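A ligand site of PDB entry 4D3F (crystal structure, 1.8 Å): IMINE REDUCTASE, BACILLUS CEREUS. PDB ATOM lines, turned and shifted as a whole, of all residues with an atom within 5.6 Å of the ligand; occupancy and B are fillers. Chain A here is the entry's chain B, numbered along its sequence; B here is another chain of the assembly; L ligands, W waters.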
ATOM      1  N   GLY A  28       0.049   7.904  16.971  1.00  0.00           N
ATOM      2  CA  GLY A  28      -0.984   8.836  17.398  1.00  0.00           C
ATOM      3  C   GLY A  28      -1.696   8.215  18.584  1.00  0.00           C
ATOM      4  O   GLY A  28      -2.468   7.299  18.477  1.00  0.00           O
ATOM      5  N   LEU A  29      -1.436   8.736  19.772  1.00  0.00           N
ATOM      6  CA  LEU A  29      -2.016   8.262  20.990  1.00  0.00           C
ATOM      7  C   LEU A  29      -2.783   9.382  21.706  1.00  0.00           C
ATOM      8  O   LEU A  29      -2.645   9.548  22.937  1.00  0.00           O
ATOM      9  CB  LEU A  29      -0.969   7.649  21.957  1.00  0.00           C
ATOM     10  CG  LEU A  29      -0.153   6.487  21.412  1.00  0.00           C
ATOM     11  CD1 LEU A  29       0.918   6.134  22.393  1.00  0.00           C
ATOM     12  CD2 LEU A  29      -1.021   5.305  21.115  1.00  0.00           C
ATOM     13  N   GLY A  30      -3.708  10.037  20.978  1.00  0.00           N
ATOM     14  CA  GLY A  30      -4.898  10.605  21.582  1.00  0.00           C
ATOM     15  C   GLY A  30      -5.800   9.546  22.129  1.00  0.00           C
ATOM     16  O   GLY A  30      -5.443   8.342  22.129  1.00  0.00           O
ATOM     17  N   PRO A  31      -6.985   9.911  22.604  1.00  0.00           N
ATOM     18  CA  PRO A  31      -7.865   8.932  23.214  1.00  0.00           C
ATOM     19  C   PRO A  31      -8.264   7.785  22.287  1.00  0.00           C
ATOM     20  O   PRO A  31      -8.426   6.632  22.733  1.00  0.00           O
ATOM     21  CB  PRO A  31      -9.117   9.742  23.552  1.00  0.00           C
ATOM     22  CG  PRO A  31      -8.573  11.147  23.741  1.00  0.00           C
ATOM     23  CD  PRO A  31      -7.408  11.314  22.893  1.00  0.00           C
ATOM     24  N   MET A  32      -8.425   8.107  21.004  1.00  0.00           N
ATOM     25  CA  MET A  32      -8.762   7.067  19.967  1.00  0.00           C
ATOM     26  C   MET A  32      -7.556   6.089  19.737  1.00  0.00           C
ATOM     27  O   MET A  32      -7.733   4.864  19.835  1.00  0.00           O
ATOM     28  CB  MET A  32      -9.105   7.703  18.647  1.00  0.00           C
ATOM     29  CG  MET A  32     -10.394   8.497  18.680  1.00  0.00           C
ATOM     30  SD  MET A  32     -11.853   7.442  18.953  1.00  0.00           S
ATOM     31  CE  MET A  32     -12.173   6.752  17.343  1.00  0.00           C
ATOM     32  N   GLY A  33      -6.358   6.625  19.513  1.00  0.00           N
ATOM     33  CA  GLY A  33      -5.189   5.793  19.334  1.00  0.00           C
ATOM     34  C   GLY A  33      -4.927   4.933  20.571  1.00  0.00           C
ATOM     35  O   GLY A  33      -4.528   3.759  20.500  1.00  0.00           O
ATOM     36  N   TRP A  50       4.101   5.068  18.795  1.00  0.00           N
ATOM     37  CA  TRP A  50       4.900   6.308  18.834  1.00  0.00           C
ATOM     38  C   TRP A  50       3.845   7.428  19.011  1.00  0.00           C
ATOM     39  O   TRP A  50       2.774   7.365  18.436  1.00  0.00           O
ATOM     40  CB  TRP A  50       5.721   6.574  17.603  1.00  0.00           C
ATOM     41  CG  TRP A  50       6.458   7.844  17.614  1.00  0.00           C
ATOM     42  CD1 TRP A  50       7.697   8.042  18.102  1.00  0.00           C
ATOM     43  CD2 TRP A  50       6.006   9.106  17.134  1.00  0.00           C
ATOM     44  NE1 TRP A  50       8.034   9.384  18.027  1.00  0.00           N
ATOM     45  CE2 TRP A  50       7.021  10.048  17.402  1.00  0.00           C
ATOM     46  CE3 TRP A  50       4.825   9.553  16.541  1.00  0.00           C
ATOM     47  CZ2 TRP A  50       6.895  11.414  17.078  1.00  0.00           C
ATOM     48  CZ3 TRP A  50       4.676  10.931  16.272  1.00  0.00           C
ATOM     49  CH2 TRP A  50       5.752  11.818  16.483  1.00  0.00           C
ATOM     50  N   ASN A  51       4.256   8.443  19.749  1.00  0.00           N
ATOM     51  CA  ASN A  51       3.477   9.635  19.928  1.00  0.00           C
ATOM     52  C   ASN A  51       4.414  10.808  20.123  1.00  0.00           C
ATOM     53  O   ASN A  51       5.485  10.668  20.693  1.00  0.00           O
ATOM     54  CB  ASN A  51       2.556   9.484  21.119  1.00  0.00           C
ATOM     55  CG  ASN A  51       1.453  10.557  21.170  1.00  0.00           C
ATOM     56  OD1 ASN A  51       1.218  11.284  22.186  1.00  0.00           O
ATOM     57  ND2 ASN A  51       0.792  10.632  20.104  1.00  0.00           N
ATOM     58  N   ARG A  52       4.036  11.965  19.637  1.00  0.00           N
ATOM     59  CA  ARG A  52       4.791  13.191  19.893  1.00  0.00           C
ATOM     60  C   ARG A  52       4.993  13.378  21.396  1.00  0.00           C
ATOM     61  O   ARG A  52       6.094  13.723  21.854  1.00  0.00           O
ATOM     62  CB  ARG A  52       4.024  14.390  19.254  1.00  0.00           C
ATOM     63  CG  ARG A  52       4.509  15.762  19.721  1.00  0.00           C
ATOM     64  CD  ARG A  52       3.708  16.841  19.023  1.00  0.00           C
ATOM     65  NE  ARG A  52       2.323  16.867  19.481  1.00  0.00           N
ATOM     66  CZ  ARG A  52       1.454  17.794  19.101  1.00  0.00           C
ATOM     67  NH1 ARG A  52       1.901  18.809  18.404  1.00  0.00           N
ATOM     68  NH2 ARG A  52       0.204  17.753  19.542  1.00  0.00           N
ATOM     69  N   THR A  53       3.948  13.207  22.159  1.00  0.00           N
ATOM     70  CA  THR A  53       3.986  13.359  23.572  1.00  0.00           C
ATOM     71  C   THR A  53       4.178  11.918  24.131  1.00  0.00           C
ATOM     72  O   THR A  53       3.211  11.164  24.351  1.00  0.00           O
ATOM     73  CB  THR A  53       2.726  14.029  24.141  1.00  0.00           C
ATOM     74  OG1 THR A  53       2.526  15.324  23.485  1.00  0.00           O
ATOM     75  CG2 THR A  53       2.792  14.124  25.643  1.00  0.00           C
ATOM     76  N   LYS A  56       2.219   9.812  27.002  1.00  0.00           N
ATOM     77  CA  LYS A  56       0.882   9.293  26.825  1.00  0.00           C
ATOM     78  C   LYS A  56       0.782   7.785  26.588  1.00  0.00           C
ATOM     79  O   LYS A  56      -0.289   7.217  26.710  1.00  0.00           O
ATOM     80  CB  LYS A  56       0.142   9.994  25.696  1.00  0.00           C
ATOM     81  CG  LYS A  56      -0.235  11.441  26.007  1.00  0.00           C
ATOM     82  CD  LYS A  56      -1.472  11.760  25.172  1.00  0.00           C
ATOM     83  CE  LYS A  56      -1.497  13.191  24.899  1.00  0.00           C
ATOM     84  NZ  LYS A  56      -2.450  13.450  23.766  1.00  0.00           N
ATOM     85  N   SER A  84      -3.794   7.585  13.946  1.00  0.00           N
ATOM     86  CA  SER A  84      -4.959   8.242  14.553  1.00  0.00           C
ATOM     87  C   SER A  84      -4.505   9.638  15.007  1.00  0.00           C
ATOM     88  O   SER A  84      -4.085   9.854  16.133  1.00  0.00           O
ATOM     89  CB  SER A  84      -5.476   7.447  15.666  1.00  0.00           C
ATOM     90  OG  SER A  84      -6.648   8.036  16.251  1.00  0.00           O
ATOM     91  N   LEU A  85      -4.449  10.500  14.051  1.00  0.00           N
ATOM     92  CA  LEU A  85      -3.924  11.871  14.267  1.00  0.00           C
ATOM     93  C   LEU A  85      -5.028  12.904  14.076  1.00  0.00           C
ATOM     94  O   LEU A  85      -6.128  12.591  13.613  1.00  0.00           O
ATOM     95  CB  LEU A  85      -2.869  12.085  13.245  1.00  0.00           C
ATOM     96  CG  LEU A  85      -1.670  11.134  13.277  1.00  0.00           C
ATOM     97  CD1 LEU A  85      -0.885  11.346  12.019  1.00  0.00           C
ATOM     98  CD2 LEU A  85      -0.878  11.359  14.556  1.00  0.00           C
ATOM     99  N   THR A  86      -4.725  14.145  14.427  1.00  0.00           N
ATOM    100  CA  THR A  86      -5.806  15.126  14.357  1.00  0.00           C
ATOM    101  C   THR A  86      -6.456  15.270  12.943  1.00  0.00           C
ATOM    102  O   THR A  86      -7.711  15.253  12.827  1.00  0.00           O
ATOM    103  CB  THR A  86      -5.375  16.465  14.977  1.00  0.00           C
ATOM    104  OG1 THR A  86      -4.961  16.196  16.323  1.00  0.00           O
ATOM    105  CG2 THR A  86      -6.561  17.422  14.965  1.00  0.00           C
ATOM    106  N   ASP A  87      -5.604  15.393  11.939  1.00  0.00           N
ATOM    107  CA  ASP A  87      -5.986  15.554  10.559  1.00  0.00           C
ATOM    108  C   ASP A  87      -4.808  15.248   9.676  1.00  0.00           C
ATOM    109  O   ASP A  87      -3.713  14.936  10.171  1.00  0.00           O
ATOM    110  CB  ASP A  87      -6.450  16.998  10.328  1.00  0.00           C
ATOM    111  CG  ASP A  87      -5.377  18.023  10.625  1.00  0.00           C
ATOM    112  OD1 ASP A  87      -4.147  17.760  10.480  1.00  0.00           O
ATOM    113  OD2 ASP A  87      -5.765  19.137  10.981  1.00  0.00           O
ATOM    114  N   VAL A  90      -1.198  16.922   9.924  1.00  0.00           N
ATOM    115  CA  VAL A  90      -0.337  16.324  10.936  1.00  0.00           C
ATOM    116  C   VAL A  90       0.426  15.175  10.276  1.00  0.00           C
ATOM    117  O   VAL A  90       1.606  14.982  10.517  1.00  0.00           O
ATOM    118  CB  VAL A  90      -1.119  15.789  12.176  1.00  0.00           C
ATOM    119  CG1 VAL A  90      -0.210  15.105  13.197  1.00  0.00           C
ATOM    120  CG2 VAL A  90      -1.902  16.885  12.859  1.00  0.00           C
ATOM    121  N   SER A  93       3.233  16.453   8.398  1.00  0.00           N
ATOM    122  CA  SER A  93       4.195  17.061   9.276  1.00  0.00           C
ATOM    123  C   SER A  93       5.147  15.990   9.805  1.00  0.00           C
ATOM    124  O   SER A  93       6.366  16.194   9.795  1.00  0.00           O
ATOM    125  CB  SER A  93       3.476  17.710  10.404  1.00  0.00           C
ATOM    126  OG  SER A  93       4.404  18.208  11.287  1.00  0.00           O
ATOM    127  N   ILE A  94       4.598  14.861  10.207  1.00  0.00           N
ATOM    128  CA  ILE A  94       5.468  13.765  10.740  1.00  0.00           C
ATOM    129  C   ILE A  94       6.087  12.828   9.726  1.00  0.00           C
ATOM    130  O   ILE A  94       7.125  12.237  10.034  1.00  0.00           O
ATOM    131  CB  ILE A  94       4.799  12.937  11.864  1.00  0.00           C
ATOM    132  CG1 ILE A  94       3.651  12.169  11.346  1.00  0.00           C
ATOM    133  CG2 ILE A  94       4.312  13.858  12.973  1.00  0.00           C
ATOM    134  CD1 ILE A  94       3.129  11.160  12.339  1.00  0.00           C
ATOM    135  N   LEU A 110      -6.958   6.789  10.053  1.00  0.00           N
ATOM    136  CA  LEU A 110      -8.249   6.889  10.759  1.00  0.00           C
ATOM    137  C   LEU A 110      -8.551   8.326  11.275  1.00  0.00           C
ATOM    138  O   LEU A 110      -9.455   8.495  12.072  1.00  0.00           O
ATOM    139  CB  LEU A 110      -8.310   5.930  11.872  1.00  0.00           C
ATOM    140  CG  LEU A 110      -8.047   4.458  11.457  1.00  0.00           C
ATOM    141  CD1 LEU A 110      -8.044   3.549  12.664  1.00  0.00           C
ATOM    142  CD2 LEU A 110      -9.044   3.961  10.418  1.00  0.00           C
ATOM    143  N   SER A 111      -7.883   9.266  10.683  1.00  0.00           N
ATOM    144  CA  SER A 111      -7.987  10.692  11.011  1.00  0.00           C
ATOM    145  C   SER A 111      -9.217  11.296  10.287  1.00  0.00           C
ATOM    146  O   SER A 111      -9.436  10.985   9.101  1.00  0.00           O
ATOM    147  CB  SER A 111      -6.722  11.385  10.613  1.00  0.00           C
ATOM    148  OG  SER A 111      -5.587  10.699  11.261  1.00  0.00           O
ATOM    149  N   SER A 112      -9.938  12.204  10.971  1.00  0.00           N
ATOM    150  CA  SER A 112     -11.068  12.937  10.351  1.00  0.00           C
ATOM    151  C   SER A 112     -10.534  14.053   9.498  1.00  0.00           C
ATOM    152  O   SER A 112      -9.736  14.848   9.938  1.00  0.00           O
ATOM    153  CB  SER A 112     -11.972  13.562  11.454  1.00  0.00           C
ATOM    154  OG  SER A 112     -12.616  12.515  12.127  1.00  0.00           O
ATOM    155  N   VAL A 137     -14.040   6.505  11.388  1.00  0.00           N
ATOM    156  CA  VAL A 137     -14.482   5.752  12.520  1.00  0.00           C
ATOM    157  C   VAL A 137     -15.780   6.370  13.053  1.00  0.00           C
ATOM    158  O   VAL A 137     -15.792   7.589  13.303  1.00  0.00           O
ATOM    159  CB  VAL A 137     -13.417   5.761  13.647  1.00  0.00           C
ATOM    160  CG1 VAL A 137     -13.902   4.957  14.857  1.00  0.00           C
ATOM    161  CG2 VAL A 137     -12.127   5.119  13.141  1.00  0.00           C
ATOM    162  N   GLN A 138     -16.798   5.555  13.289  1.00  0.00           N
ATOM    163  CA  GLN A 138     -18.146   6.124  13.594  1.00  0.00           C
ATOM    164  C   GLN A 138     -18.503   6.217  15.093  1.00  0.00           C
ATOM    165  O   GLN A 138     -19.668   6.447  15.460  1.00  0.00           O
ATOM    166  CB  GLN A 138     -19.212   5.262  12.876  1.00  0.00           C
ATOM    167  CG  GLN A 138     -19.148   5.372  11.376  1.00  0.00           C
ATOM    168  CD  GLN A 138     -20.031   4.364  10.723  1.00  0.00           C
ATOM    169  OE1 GLN A 138     -21.052   4.017  11.257  1.00  0.00           O
ATOM    170  NE2 GLN A 138     -19.557   3.754   9.640  1.00  0.00           N
ATOM    171  N   VAL A 139     -17.534   5.942  15.956  1.00  0.00           N
ATOM    172  CA  VAL A 139     -17.754   5.756  17.368  1.00  0.00           C
ATOM    173  C   VAL A 139     -16.643   6.434  18.192  1.00  0.00           C
ATOM    174  O   VAL A 139     -15.513   6.666  17.696  1.00  0.00           O
ATOM    175  CB  VAL A 139     -17.861   4.286  17.802  1.00  0.00           C
ATOM    176  CG1 VAL A 139     -19.044   3.584  17.147  1.00  0.00           C
ATOM    177  CG2 VAL A 139     -16.513   3.510  17.582  1.00  0.00           C
ATOM    178  N   PRO A 140     -16.947   6.767  19.461  1.00  0.00           N
ATOM    179  CA  PRO A 140     -15.937   7.311  20.333  1.00  0.00           C
ATOM    180  C   PRO A 140     -15.003   6.209  20.817  1.00  0.00           C
ATOM    181  O   PRO A 140     -15.248   5.039  20.503  1.00  0.00           O
ATOM    182  CB  PRO A 140     -16.756   7.901  21.492  1.00  0.00           C
ATOM    183  CG  PRO A 140     -17.968   7.111  21.539  1.00  0.00           C
ATOM    184  CD  PRO A 140     -18.281   6.737  20.108  1.00  0.00           C
ATOM    185  N   PRO A 141     -13.973   6.564  21.602  1.00  0.00           N
ATOM    186  CA  PRO A 141     -13.028   5.533  22.139  1.00  0.00           C
ATOM    187  C   PRO A 141     -13.670   4.367  22.790  1.00  0.00           C
ATOM    188  O   PRO A 141     -13.238   3.240  22.550  1.00  0.00           O
ATOM    189  CB  PRO A 141     -12.110   6.327  23.076  1.00  0.00           C
ATOM    190  CG  PRO A 141     -12.145   7.730  22.493  1.00  0.00           C
ATOM    191  CD  PRO A 141     -13.522   7.926  21.958  1.00  0.00           C
ATOM    192  N   TYR A 187     -18.472   9.711   6.126  1.00  0.00           N
ATOM    193  CA  TYR A 187     -18.339  10.253   7.424  1.00  0.00           C
ATOM    194  C   TYR A 187     -18.815  11.717   7.494  1.00  0.00           C
ATOM    195  O   TYR A 187     -19.619  12.024   8.397  1.00  0.00           O
ATOM    196  CB  TYR A 187     -16.885  10.156   7.886  1.00  0.00           C
ATOM    197  CG  TYR A 187     -16.660  10.684   9.284  1.00  0.00           C
ATOM    198  CD1 TYR A 187     -16.944   9.881  10.409  1.00  0.00           C
ATOM    199  CD2 TYR A 187     -16.237  12.011   9.503  1.00  0.00           C
ATOM    200  CE1 TYR A 187     -16.716  10.360  11.675  1.00  0.00           C
ATOM    201  CE2 TYR A 187     -16.047  12.510  10.788  1.00  0.00           C
ATOM    202  CZ  TYR A 187     -16.290  11.685  11.843  1.00  0.00           C
ATOM    203  OH  TYR A 187     -16.117  12.132  13.089  1.00  0.00           O
ATOM    204  N   MET B 254     -13.990  20.693  20.266  1.00  0.00           N
ATOM    205  CA  MET B 254     -13.880  19.557  19.376  1.00  0.00           C
ATOM    206  C   MET B 254     -15.091  19.480  18.406  1.00  0.00           C
ATOM    207  O   MET B 254     -14.947  19.099  17.248  1.00  0.00           O
ATOM    208  CB  MET B 254     -13.769  18.218  20.146  1.00  0.00           C
ATOM    209  CG  MET B 254     -12.504  18.080  20.980  1.00  0.00           C
ATOM    210  SD  MET B 254     -11.059  18.349  19.903  1.00  0.00           S
ATOM    211  CE  MET B 254     -10.400  16.678  19.837  1.00  0.00           C
HETATM  212  P1  LIG L   1      -6.384  14.158  19.176  1.00  0.00           P
HETATM  213  O1  LIG L   1      -6.322  14.985  20.441  1.00  0.00           O
HETATM  214  O2  LIG L   1      -6.844  14.681  17.850  1.00  0.00           O
HETATM  215  O3  LIG L   1      -4.844  13.751  18.980  1.00  0.00           O
HETATM  216  C1  LIG L   1      -4.525  12.820  17.990  1.00  0.00           C
HETATM  217  C2  LIG L   1      -3.034  12.690  17.859  1.00  0.00           C
HETATM  218  O4  LIG L   1      -2.538  13.651  16.922  1.00  0.00           O
HETATM  219  C3  LIG L   1      -2.259  12.763  19.144  1.00  0.00           C
HETATM  220  O5  LIG L   1      -1.297  11.725  19.003  1.00  0.00           O
HETATM  221  C4  LIG L   1      -1.494  14.054  18.961  1.00  0.00           C
HETATM  222  O6  LIG L   1      -0.192  14.130  19.604  1.00  0.00           O
HETATM  223  C5  LIG L   1      -1.322  14.073  17.473  1.00  0.00           C
HETATM  224  N1  LIG L   1      -0.971  15.391  16.943  1.00  0.00           N
HETATM  225  C6  LIG L   1      -1.791  16.459  16.910  1.00  0.00           C
HETATM  226  N2  LIG L   1      -1.101  17.449  16.314  1.00  0.00           N
HETATM  227  C7  LIG L   1       0.126  17.005  16.044  1.00  0.00           C
HETATM  228  C8  LIG L   1       1.336  17.555  15.494  1.00  0.00           C
HETATM  229  N3  LIG L   1       1.247  18.829  15.098  1.00  0.00           N
HETATM  230  N4  LIG L   1       2.431  16.827  15.332  1.00  0.00           N
HETATM  231  C9  LIG L   1       2.468  15.526  15.729  1.00  0.00           C
HETATM  232  N5  LIG L   1       1.380  14.934  16.298  1.00  0.00           N
HETATM  233  C10 LIG L   1       0.198  15.622  16.433  1.00  0.00           C
HETATM  234  O7  LIG L   1      -7.077  12.846  19.633  1.00  0.00           O
HETATM  235  P2  LIG L   1      -8.286  11.886  19.190  1.00  0.00           P
HETATM  236  O8  LIG L   1      -9.475  12.240  19.971  1.00  0.00           O
HETATM  237  O9  LIG L   1      -7.826  10.512  19.608  1.00  0.00           O
HETATM  238  O10 LIG L   1      -8.504  12.082  17.655  1.00  0.00           O
HETATM  239  C11 LIG L   1      -7.812  11.463  16.536  1.00  0.00           C
HETATM  240  C12 LIG L   1      -8.671  11.429  15.298  1.00  0.00           C
HETATM  241  O11 LIG L   1      -9.795  10.575  15.508  1.00  0.00           O
HETATM  242  C13 LIG L   1      -9.288  12.814  14.992  1.00  0.00           C
HETATM  243  O12 LIG L   1      -9.095  13.053  13.582  1.00  0.00           O
HETATM  244  C14 LIG L   1     -10.723  12.736  15.489  1.00  0.00           C
HETATM  245  O13 LIG L   1     -11.607  13.590  14.771  1.00  0.00           O
HETATM  246  C15 LIG L   1     -10.997  11.258  15.143  1.00  0.00           C
HETATM  247  N6  LIG L   1     -12.142  10.725  15.801  1.00  0.00           N
HETATM  248  C16 LIG L   1     -12.303  10.990  17.114  1.00  0.00           C
HETATM  249  C17 LIG L   1     -13.399  10.539  17.811  1.00  0.00           C
HETATM  250  C18 LIG L   1     -13.436  10.837  19.290  1.00  0.00           C
HETATM  251  O14 LIG L   1     -14.462  10.560  19.837  1.00  0.00           O
HETATM  252  N7  LIG L   1     -12.353  11.155  20.031  1.00  0.00           N
HETATM  253  C19 LIG L   1     -14.382   9.804  17.147  1.00  0.00           C
HETATM  254  C20 LIG L   1     -14.219   9.518  15.780  1.00  0.00           C
HETATM  255  C21 LIG L   1     -13.080   9.974  15.099  1.00  0.00           C
HETATM  256  P3  LIG L   1      -0.106  14.488  21.161  1.00  0.00           P
HETATM  257  O15 LIG L   1       1.372  14.732  21.282  1.00  0.00           O
HETATM  258  O16 LIG L   1      -1.024  15.753  21.327  1.00  0.00           O
HETATM  259  O17 LIG L   1      -0.705  13.300  21.926  1.00  0.00           O
HETATM  260  O   HOH W   1      -5.456   9.242  18.775  1.00  0.00           O
HETATM  261  O   HOH W   2     -11.073  14.130  18.537  1.00  0.00           O
HETATM  262  O   HOH W   3      -4.940  14.262  22.629  1.00  0.00           O
HETATM  263  O   HOH W   4       1.812  12.142  17.703  1.00  0.00           O
HETATM  264  O   HOH W   5      -9.499  14.340  21.851  1.00  0.00           O
HETATM  265  O   HOH W   6      -8.988   8.080  14.909  1.00  0.00           O
HETATM  266  O   HOH W   7     -14.857  11.264  22.532  1.00  0.00           O
HETATM  267  O   HOH W   8     -13.103  16.437  13.885  1.00  0.00           O
HETATM  268  O   HOH W   9     -17.389   9.344  14.912  1.00  0.00           O
HETATM  269  O   HOH W  10      -9.120  15.783  17.364  1.00  0.00           O
HETATM  270  O   HOH W  11       4.933  17.641  15.102  1.00  0.00           O
HETATM  271  O   HOH W  12     -12.155  11.745  23.160  1.00  0.00           O
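O of Thr 53 lies close to OD1 of Asn 51 (2.9 Å).
The side-chain amide nitrogen (ND2) of Asn 51 sits close to the backbone NH (N) of Leu 29 (2.9 Å).
N of Leu 85 is in hydrogen-bond range of OG of Ser 111, 3.0 Å away.
The backbone NH of Val 90 is in hydrogen-bond range of the side-chain carboxylate of Asp 87, at 3.1 Å.
The backbone NH (N) of Gly 28 sits at hydrogen-bond distance from the backbone carbonyl oxygen (O) of Trp 50 (3.1 Å).
Water W3 bridges an oxygen (O1) of the ligand (2.7 Å) and the side-chain amino group of Lys 56 (2.9 Å).
Water W6 lies within hydrogen-bond range of O11 of the ligand, OG of Ser 84 and O of Leu 110.
Water W1 lies within hydrogen-bond range of O9 of the ligand (2.8 Å), N of Gly 33 (2.9 Å), N of Gly 30 (2.9 Å) and O of Ser 84 (3.0 Å).
Water W4 lies within hydrogen-bond range of N of Arg 52 (3.0 Å), ND2 of Asn 51 (3.0 Å) and N5 of the ligand (3.2 Å).
N of Pro 31 sits close to O9 of the ligand (3.2 Å).
CA of Gly 28 touches O5 of the ligand (3.3 Å).
Gly 30 touches the ligand (C to O9, 3.4 Å).
Ser 84 touches the ligand.
CG1 of Val 90 touches C10 of the ligand, at 3.3 Å.
Ile 94 touches the ligand.
CA of Ser 111 touches O12 of the ligand (3.7 Å).
Val 137 touches the ligand.
Val 139 touches the ligand (O to C19, 3.4 Å).
Pro 140 touches the ligand (CA to O14, 3.6 Å).
Pro 141 touches the ligand (CD to O14, 3.5 Å).
Hydrophobic or aromatic side chains within 4 Å of the ligand: Pro 31, Met 32, Leu 85, Val 90, Ile 94, Pro 140 and Pro 141.
Of the 28 residues printed, 20 come within 4 Å of the ligand.
Along chain A the residues within 4 Å of the ligand span positions 28 to 141.
The nearest printed residue that does not touch the ligand is Leu 110 (4.03 Å).
NZ of Lys 56 is in salt-bridge range of O17 of the ligand, at 2.5 Å.
O15 of the ligand is in hydrogen-bond range of N of Thr 53 (3.1 Å).
The side-chain hydroxyl of Thr 53 is in hydrogen-bond range of an oxygen (O15) of the ligand.
An oxygen (O5) of the ligand is in hydrogen-bond range of the side-chain amide nitrogen (ND2) of Asn 51 (2.6 Å).
The backbone NH (N) of Thr 86 sits at hydrogen-bond distance from an oxygen (O4) of the ligand (3.4 Å).
O of Thr 86 lies within hydrogen-bond range of O12 of the ligand (2.7 Å).
The side-chain hydroxyl (OG1) of Thr 86 sits at hydrogen-bond distance from an oxygen (O2) of the ligand (2.9 Å).
O9 of the ligand lies within hydrogen-bond range of N of Met 32 (2.8 Å).
N of Ser 112 is in hydrogen-bond range of O12 of the ligand (2.9 Å).
The side-chain hydroxyl of Ser 112 is in hydrogen-bond range of an oxygen (O13) of the ligand, at 3.0 Å.
NH2 of Arg 52 is in salt-bridge range of O16 of the ligand (2.9 Å).
O of Leu 85 lies within hydrogen-bond range of O12 of the ligand, 3.0 Å away.
O5 of the ligand is in hydrogen-bond range of N of Leu 29.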
